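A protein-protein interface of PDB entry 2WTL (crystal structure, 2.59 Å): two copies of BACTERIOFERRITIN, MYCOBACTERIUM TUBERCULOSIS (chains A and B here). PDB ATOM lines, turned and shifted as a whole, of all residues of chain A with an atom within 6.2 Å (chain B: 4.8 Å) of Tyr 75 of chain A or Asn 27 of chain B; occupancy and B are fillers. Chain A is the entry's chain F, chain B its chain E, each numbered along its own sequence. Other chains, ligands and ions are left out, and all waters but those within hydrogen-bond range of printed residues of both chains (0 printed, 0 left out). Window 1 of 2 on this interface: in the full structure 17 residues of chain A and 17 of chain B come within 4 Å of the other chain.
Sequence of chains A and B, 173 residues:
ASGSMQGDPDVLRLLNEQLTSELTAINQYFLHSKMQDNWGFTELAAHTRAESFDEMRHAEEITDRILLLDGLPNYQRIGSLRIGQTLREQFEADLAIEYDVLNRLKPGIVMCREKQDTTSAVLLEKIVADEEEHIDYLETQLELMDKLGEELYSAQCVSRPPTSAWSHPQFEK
ND2 of Asn 27 of chain B sits at hydrogen-bond distance from O of Tyr 75 of chain A (3.0 Å). The backbone NH (N) of Leu 81 of chain B lies close to the side-chain amide nitrogen (NE2) of Gln 76 of chain A, at 2.8 Å.
OH of Tyr 75 of chain A is in hydrogen-bond range of OG1 of Thr 63 of chain A (2.7 Å). The side-chain amide oxygen of Asn 74 of chain A lies within hydrogen-bond range of the backbone NH of Gln 76 of chain A (2.9 Å).
Phe 30 of chain B touches Glu 60 of chain A (CZ to OE2, 3.8 Å). CG of Pro 73 of chain A touches CD1 of Leu 31 of chain B (3.8 Å). Tyr 75 of chain A touches Phe 30 of chain B. CD1 of Ile 78 of chain B touches O of Tyr 75 of chain A (3.9 Å). Leu 81 of chain B touches Tyr 75 of chain A. Ile 78 of chain B touches Gln 76 of chain A (CD1 to O, 3.8 Å).
Of the printed residues of chain B, Tyr 75 of chain A touches Asn 27 (3.0 Å), Phe 30 (3.2 Å), Ile 78 (3.9 Å) and Leu 81 (3.1 Å). Asn 27 of chain B touches one residue of chain A. Printed residues of chain B within 4 Å of Gln 76 of chain A: Ile 78 (3.8 Å) and Leu 81 (2.8 Å). Of the printed residues of chain B, Glu 60 of chain A touches Phe 30. The nearest printed residue of chain A that does not touch Phe 30 of chain B is Thr 63 of chain A (4.8 Å).
Hydrophobic or aromatic side chains of chain B within 4 Å of the printed part of chain A: Phe 30, Leu 31, Ile 78 and Leu 81. Of the 11 printed residues of chain A, 4 touch a printed residue of chain B. Hydrophobic or aromatic side chains of chain A within 4 Å of the printed part of chain B: Pro 73 and Tyr 75. Along chain A the printed residues that touch a printed residue of chain B span positions 60 to 76. Among the printed residues, 8 pairs touch across the chains. Among the printed residues, no Asp or Glu carboxylate lies within 4 Å of a Lys or Arg side-chain nitrogen of the other chain.
Position printed for both chains: 23. Of the 8 pairs that touch across the chains among the printed residues, none has its exchanged pair printed and touching as well.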
ATOM      1  N   ASN A  16     -28.197  31.410   3.862  1.00  0.00           N
ATOM      2  CA  ASN A  16     -28.171  30.058   3.312  1.00  0.00           C
ATOM      3  C   ASN A  16     -29.028  29.904   2.063  1.00  0.00           C
ATOM      4  O   ASN A  16     -28.716  29.116   1.168  1.00  0.00           O
ATOM      5  CB  ASN A  16     -28.587  29.033   4.361  1.00  0.00           C
ATOM      6  CG  ASN A  16     -27.402  28.390   5.035  1.00  0.00           C
ATOM      7  OD1 ASN A  16     -26.459  27.952   4.369  1.00  0.00           O
ATOM      8  ND2 ASN A  16     -27.431  28.336   6.362  1.00  0.00           N
ATOM      9  N   LEU A  19     -27.075  31.354  -0.658  1.00  0.00           N
ATOM     10  CA  LEU A  19     -26.005  30.413  -0.959  1.00  0.00           C
ATOM     11  C   LEU A  19     -26.479  29.317  -1.904  1.00  0.00           C
ATOM     12  O   LEU A  19     -25.776  28.953  -2.842  1.00  0.00           O
ATOM     13  CB  LEU A  19     -25.438  29.792   0.324  1.00  0.00           C
ATOM     14  CG  LEU A  19     -24.307  28.771   0.126  1.00  0.00           C
ATOM     15  CD1 LEU A  19     -23.152  29.368  -0.674  1.00  0.00           C
ATOM     16  CD2 LEU A  19     -23.814  28.207   1.458  1.00  0.00           C
ATOM     17  N   LEU A  23     -25.066  28.468  -5.728  1.00  0.00           N
ATOM     18  CA  LEU A  23     -24.581  27.175  -6.206  1.00  0.00           C
ATOM     19  C   LEU A  23     -25.314  26.785  -7.473  1.00  0.00           C
ATOM     20  O   LEU A  23     -24.724  26.226  -8.396  1.00  0.00           O
ATOM     21  CB  LEU A  23     -24.756  26.086  -5.146  1.00  0.00           C
ATOM     22  CG  LEU A  23     -24.083  26.305  -3.790  1.00  0.00           C
ATOM     23  CD1 LEU A  23     -24.185  25.049  -2.933  1.00  0.00           C
ATOM     24  CD2 LEU A  23     -22.634  26.711  -3.964  1.00  0.00           C
ATOM     25  N   ALA A  59     -20.450  33.086  -3.688  1.00  0.00           N
ATOM     26  CA  ALA A  59     -20.643  31.892  -2.872  1.00  0.00           C
ATOM     27  C   ALA A  59     -19.674  31.836  -1.695  1.00  0.00           C
ATOM     28  O   ALA A  59     -20.063  31.477  -0.582  1.00  0.00           O
ATOM     29  CB  ALA A  59     -20.509  30.641  -3.727  1.00  0.00           C
ATOM     30  N   GLU A  60     -18.416  32.192  -1.935  1.00  0.00           N
ATOM     31  CA  GLU A  60     -17.414  32.144  -0.880  1.00  0.00           C
ATOM     32  C   GLU A  60     -17.604  33.238   0.172  1.00  0.00           C
ATOM     33  O   GLU A  60     -17.482  32.980   1.373  1.00  0.00           O
ATOM     34  CB  GLU A  60     -15.998  32.201  -1.447  1.00  0.00           C
ATOM     35  CG  GLU A  60     -14.952  32.189  -0.348  1.00  0.00           C
ATOM     36  CD  GLU A  60     -13.555  31.955  -0.855  1.00  0.00           C
ATOM     37  OE1 GLU A  60     -13.234  32.417  -1.969  1.00  0.00           O
ATOM     38  OE2 GLU A  60     -12.772  31.305  -0.136  1.00  0.00           O
ATOM     39  N   THR A  63     -20.362  32.240   2.358  1.00  0.00           N
ATOM     40  CA  THR A  63     -19.869  31.153   3.195  1.00  0.00           C
ATOM     41  C   THR A  63     -19.080  31.707   4.378  1.00  0.00           C
ATOM     42  O   THR A  63     -19.260  31.279   5.516  1.00  0.00           O
ATOM     43  CB  THR A  63     -18.980  30.189   2.382  1.00  0.00           C
ATOM     44  OG1 THR A  63     -19.728  29.674   1.277  1.00  0.00           O
ATOM     45  CG2 THR A  63     -18.499  29.029   3.239  1.00  0.00           C
ATOM     46  N   PRO A  73     -22.810  26.433   6.775  1.00  0.00           N
ATOM     47  CA  PRO A  73     -23.177  26.711   5.383  1.00  0.00           C
ATOM     48  C   PRO A  73     -23.767  25.475   4.715  1.00  0.00           C
ATOM     49  O   PRO A  73     -23.254  24.371   4.892  1.00  0.00           O
ATOM     50  CB  PRO A  73     -21.839  27.089   4.734  1.00  0.00           C
ATOM     51  CG  PRO A  73     -20.921  27.425   5.875  1.00  0.00           C
ATOM     52  CD  PRO A  73     -21.360  26.549   7.001  1.00  0.00           C
ATOM     53  N   ASN A  74     -24.842  25.667   3.957  1.00  0.00           N
ATOM     54  CA  ASN A  74     -25.501  24.564   3.275  1.00  0.00           C
ATOM     55  C   ASN A  74     -24.949  24.328   1.874  1.00  0.00           C
ATOM     56  O   ASN A  74     -25.246  25.079   0.949  1.00  0.00           O
ATOM     57  CB  ASN A  74     -27.004  24.812   3.215  1.00  0.00           C
ATOM     58  CG  ASN A  74     -27.783  23.586   2.787  1.00  0.00           C
ATOM     59  OD1 ASN A  74     -27.276  22.730   2.063  1.00  0.00           O
ATOM     60  ND2 ASN A  74     -29.031  23.500   3.229  1.00  0.00           N
ATOM     61  N   TYR A  75     -24.147  23.279   1.729  1.00  0.00           N
ATOM     62  CA  TYR A  75     -23.582  22.886   0.441  1.00  0.00           C
ATOM     63  C   TYR A  75     -24.220  21.600  -0.089  1.00  0.00           C
ATOM     64  O   TYR A  75     -23.715  20.992  -1.029  1.00  0.00           O
ATOM     65  CB  TYR A  75     -22.071  22.690   0.568  1.00  0.00           C
ATOM     66  CG  TYR A  75     -21.263  23.953   0.392  1.00  0.00           C
ATOM     67  CD1 TYR A  75     -21.228  24.926   1.381  1.00  0.00           C
ATOM     68  CD2 TYR A  75     -20.533  24.172  -0.763  1.00  0.00           C
ATOM     69  CE1 TYR A  75     -20.488  26.080   1.222  1.00  0.00           C
ATOM     70  CE2 TYR A  75     -19.788  25.320  -0.933  1.00  0.00           C
ATOM     71  CZ  TYR A  75     -19.768  26.272   0.060  1.00  0.00           C
ATOM     72  OH  TYR A  75     -19.024  27.416  -0.119  1.00  0.00           O
ATOM     73  N   GLN A  76     -25.328  21.193   0.520  1.00  0.00           N
ATOM     74  CA  GLN A  76     -25.987  19.941   0.177  1.00  0.00           C
ATOM     75  C   GLN A  76     -27.151  20.167  -0.783  1.00  0.00           C
ATOM     76  O   GLN A  76     -27.518  19.282  -1.556  1.00  0.00           O
ATOM     77  CB  GLN A  76     -26.503  19.269   1.451  1.00  0.00           C
ATOM     78  CG  GLN A  76     -27.200  17.940   1.223  1.00  0.00           C
ATOM     79  CD  GLN A  76     -26.266  16.877   0.683  1.00  0.00           C
ATOM     80  OE1 GLN A  76     -26.045  16.784  -0.525  1.00  0.00           O
ATOM     81  NE2 GLN A  76     -25.715  16.062   1.579  1.00  0.00           N
ATOM     82  N   ARG A  77     -27.721  21.366  -0.728  1.00  0.00           N
ATOM     83  CA  ARG A  77     -28.954  21.679  -1.433  1.00  0.00           C
ATOM     84  C   ARG A  77     -28.682  22.485  -2.699  1.00  0.00           C
ATOM     85  O   ARG A  77     -27.997  23.509  -2.657  1.00  0.00           O
ATOM     86  CB  ARG A  77     -29.869  22.480  -0.505  1.00  0.00           C
ATOM     87  CG  ARG A  77     -31.245  22.774  -1.060  1.00  0.00           C
ATOM     88  CD  ARG A  77     -32.087  23.472  -0.008  1.00  0.00           C
ATOM     89  NE  ARG A  77     -31.529  24.776   0.339  1.00  0.00           N
ATOM     90  CZ  ARG A  77     -31.746  25.402   1.490  1.00  0.00           C
ATOM     91  NH1 ARG A  77     -32.502  24.831   2.422  1.00  0.00           N
ATOM     92  NH2 ARG A  77     -31.198  26.594   1.717  1.00  0.00           N
ATOM     93  N   LEU B  23     -18.576  16.600  -8.219  1.00  0.00           N
ATOM     94  CA  LEU B  23     -19.275  17.756  -7.667  1.00  0.00           C
ATOM     95  C   LEU B  23     -19.487  17.604  -6.162  1.00  0.00           C
ATOM     96  O   LEU B  23     -19.476  18.587  -5.420  1.00  0.00           O
ATOM     97  CB  LEU B  23     -20.615  17.960  -8.377  1.00  0.00           C
ATOM     98  CG  LEU B  23     -20.548  18.224  -9.880  1.00  0.00           C
ATOM     99  CD1 LEU B  23     -21.946  18.389 -10.444  1.00  0.00           C
ATOM    100  CD2 LEU B  23     -19.706  19.453 -10.175  1.00  0.00           C
ATOM    101  N   THR B  24     -19.682  16.366  -5.718  1.00  0.00           N
ATOM    102  CA  THR B  24     -19.805  16.075  -4.296  1.00  0.00           C
ATOM    103  C   THR B  24     -18.486  16.350  -3.583  1.00  0.00           C
ATOM    104  O   THR B  24     -18.452  17.039  -2.563  1.00  0.00           O
ATOM    105  CB  THR B  24     -20.210  14.609  -4.051  1.00  0.00           C
ATOM    106  OG1 THR B  24     -21.464  14.339  -4.693  1.00  0.00           O
ATOM    107  CG2 THR B  24     -20.338  14.332  -2.561  1.00  0.00           C
ATOM    108  N   ALA B  25     -17.402  15.810  -4.131  1.00  0.00           N
ATOM    109  CA  ALA B  25     -16.073  15.981  -3.554  1.00  0.00           C
ATOM    110  C   ALA B  25     -15.666  17.450  -3.503  1.00  0.00           C
ATOM    111  O   ALA B  25     -15.068  17.906  -2.530  1.00  0.00           O
ATOM    112  CB  ALA B  25     -15.044  15.172  -4.335  1.00  0.00           C
ATOM    113  N   ILE B  26     -15.997  18.187  -4.557  1.00  0.00           N
ATOM    114  CA  ILE B  26     -15.689  19.607  -4.623  1.00  0.00           C
ATOM    115  C   ILE B  26     -16.335  20.361  -3.469  1.00  0.00           C
ATOM    116  O   ILE B  26     -15.657  21.087  -2.743  1.00  0.00           O
ATOM    117  CB  ILE B  26     -16.148  20.223  -5.956  1.00  0.00           C
ATOM    118  CG1 ILE B  26     -15.328  19.651  -7.110  1.00  0.00           C
ATOM    119  CG2 ILE B  26     -16.044  21.744  -5.907  1.00  0.00           C
ATOM    120  CD1 ILE B  26     -15.915  19.936  -8.463  1.00  0.00           C
ATOM    121  N   ASN B  27     -17.642  20.188  -3.299  1.00  0.00           N
ATOM    122  CA  ASN B  27     -18.358  20.847  -2.212  1.00  0.00           C
ATOM    123  C   ASN B  27     -17.857  20.415  -0.838  1.00  0.00           C
ATOM    124  O   ASN B  27     -17.619  21.246   0.036  1.00  0.00           O
ATOM    125  CB  ASN B  27     -19.863  20.595  -2.312  1.00  0.00           C
ATOM    126  CG  ASN B  27     -20.535  21.440  -3.377  1.00  0.00           C
ATOM    127  OD1 ASN B  27     -19.877  22.127  -4.162  1.00  0.00           O
ATOM    128  ND2 ASN B  27     -21.859  21.393  -3.408  1.00  0.00           N
ATOM    129  N   GLN B  28     -17.703  19.110  -0.645  1.00  0.00           N
ATOM    130  CA  GLN B  28     -17.245  18.598   0.636  1.00  0.00           C
ATOM    131  C   GLN B  28     -15.849  19.120   0.985  1.00  0.00           C
ATOM    132  O   GLN B  28     -15.637  19.646   2.081  1.00  0.00           O
ATOM    133  CB  GLN B  28     -17.282  17.067   0.662  1.00  0.00           C
ATOM    134  CG  GLN B  28     -16.754  16.463   1.957  1.00  0.00           C
ATOM    135  CD  GLN B  28     -17.079  14.989   2.097  1.00  0.00           C
ATOM    136  OE1 GLN B  28     -18.211  14.569   1.871  1.00  0.00           O
ATOM    137  NE2 GLN B  28     -16.089  14.198   2.478  1.00  0.00           N
ATOM    138  N   TYR B  29     -14.903  18.976   0.056  1.00  0.00           N
ATOM    139  CA  TYR B  29     -13.532  19.417   0.305  1.00  0.00           C
ATOM    140  C   TYR B  29     -13.481  20.916   0.559  1.00  0.00           C
ATOM    141  O   TYR B  29     -12.833  21.368   1.500  1.00  0.00           O
ATOM    142  CB  TYR B  29     -12.599  19.068  -0.858  1.00  0.00           C
ATOM    143  CG  TYR B  29     -12.445  17.591  -1.121  1.00  0.00           C
ATOM    144  CD1 TYR B  29     -12.836  16.650  -0.178  1.00  0.00           C
ATOM    145  CD2 TYR B  29     -11.891  17.135  -2.307  1.00  0.00           C
ATOM    146  CE1 TYR B  29     -12.693  15.295  -0.419  1.00  0.00           C
ATOM    147  CE2 TYR B  29     -11.739  15.786  -2.553  1.00  0.00           C
ATOM    148  CZ  TYR B  29     -12.142  14.873  -1.610  1.00  0.00           C
ATOM    149  OH  TYR B  29     -11.988  13.530  -1.865  1.00  0.00           O
ATOM    150  N   PHE B  30     -14.167  21.687  -0.278  1.00  0.00           N
ATOM    151  CA  PHE B  30     -14.160  23.134  -0.115  1.00  0.00           C
ATOM    152  C   PHE B  30     -14.653  23.555   1.264  1.00  0.00           C
ATOM    153  O   PHE B  30     -13.994  24.337   1.951  1.00  0.00           O
ATOM    154  CB  PHE B  30     -14.971  23.838  -1.203  1.00  0.00           C
ATOM    155  CG  PHE B  30     -14.897  25.338  -1.123  1.00  0.00           C
ATOM    156  CD1 PHE B  30     -13.754  26.006  -1.520  1.00  0.00           C
ATOM    157  CD2 PHE B  30     -15.956  26.077  -0.626  1.00  0.00           C
ATOM    158  CE1 PHE B  30     -13.673  27.383  -1.438  1.00  0.00           C
ATOM    159  CE2 PHE B  30     -15.879  27.460  -0.543  1.00  0.00           C
ATOM    160  CZ  PHE B  30     -14.737  28.110  -0.948  1.00  0.00           C
ATOM    161  N   LEU B  31     -15.812  23.041   1.667  1.00  0.00           N
ATOM    162  CA  LEU B  31     -16.370  23.394   2.968  1.00  0.00           C
ATOM    163  C   LEU B  31     -15.411  23.027   4.107  1.00  0.00           C
ATOM    164  O   LEU B  31     -15.122  23.852   4.975  1.00  0.00           O
ATOM    165  CB  LEU B  31     -17.739  22.743   3.170  1.00  0.00           C
ATOM    166  CG  LEU B  31     -18.467  23.110   4.464  1.00  0.00           C
ATOM    167  CD1 LEU B  31     -18.749  24.603   4.525  1.00  0.00           C
ATOM    168  CD2 LEU B  31     -19.754  22.310   4.607  1.00  0.00           C
ATOM    169  N   ILE B  78     -26.246  16.304  -6.571  1.00  0.00           N
ATOM    170  CA  ILE B  78     -25.120  16.217  -5.654  1.00  0.00           C
ATOM    171  C   ILE B  78     -25.298  14.978  -4.797  1.00  0.00           C
ATOM    172  O   ILE B  78     -26.420  14.625  -4.440  1.00  0.00           O
ATOM    173  CB  ILE B  78     -25.020  17.425  -4.711  1.00  0.00           C
ATOM    174  CG1 ILE B  78     -25.334  18.731  -5.434  1.00  0.00           C
ATOM    175  CG2 ILE B  78     -23.628  17.511  -4.111  1.00  0.00           C
ATOM    176  CD1 ILE B  78     -25.224  19.943  -4.515  1.00  0.00           C
ATOM    177  N   LEU B  81     -23.446  14.488   1.745  1.00  0.00           N
ATOM    178  CA  LEU B  81     -22.379  15.315   2.295  1.00  0.00           C
ATOM    179  C   LEU B  81     -21.988  14.870   3.700  1.00  0.00           C
ATOM    180  O   LEU B  81     -22.749  15.045   4.652  1.00  0.00           O
ATOM    181  CB  LEU B  81     -22.795  16.789   2.307  1.00  0.00           C
ATOM    182  CG  LEU B  81     -21.956  17.736   1.449  1.00  0.00           C
ATOM    183  CD1 LEU B  81     -21.578  17.078   0.131  1.00  0.00           C
ATOM    184  CD2 LEU B  81     -22.698  19.042   1.208  1.00  0.00           C
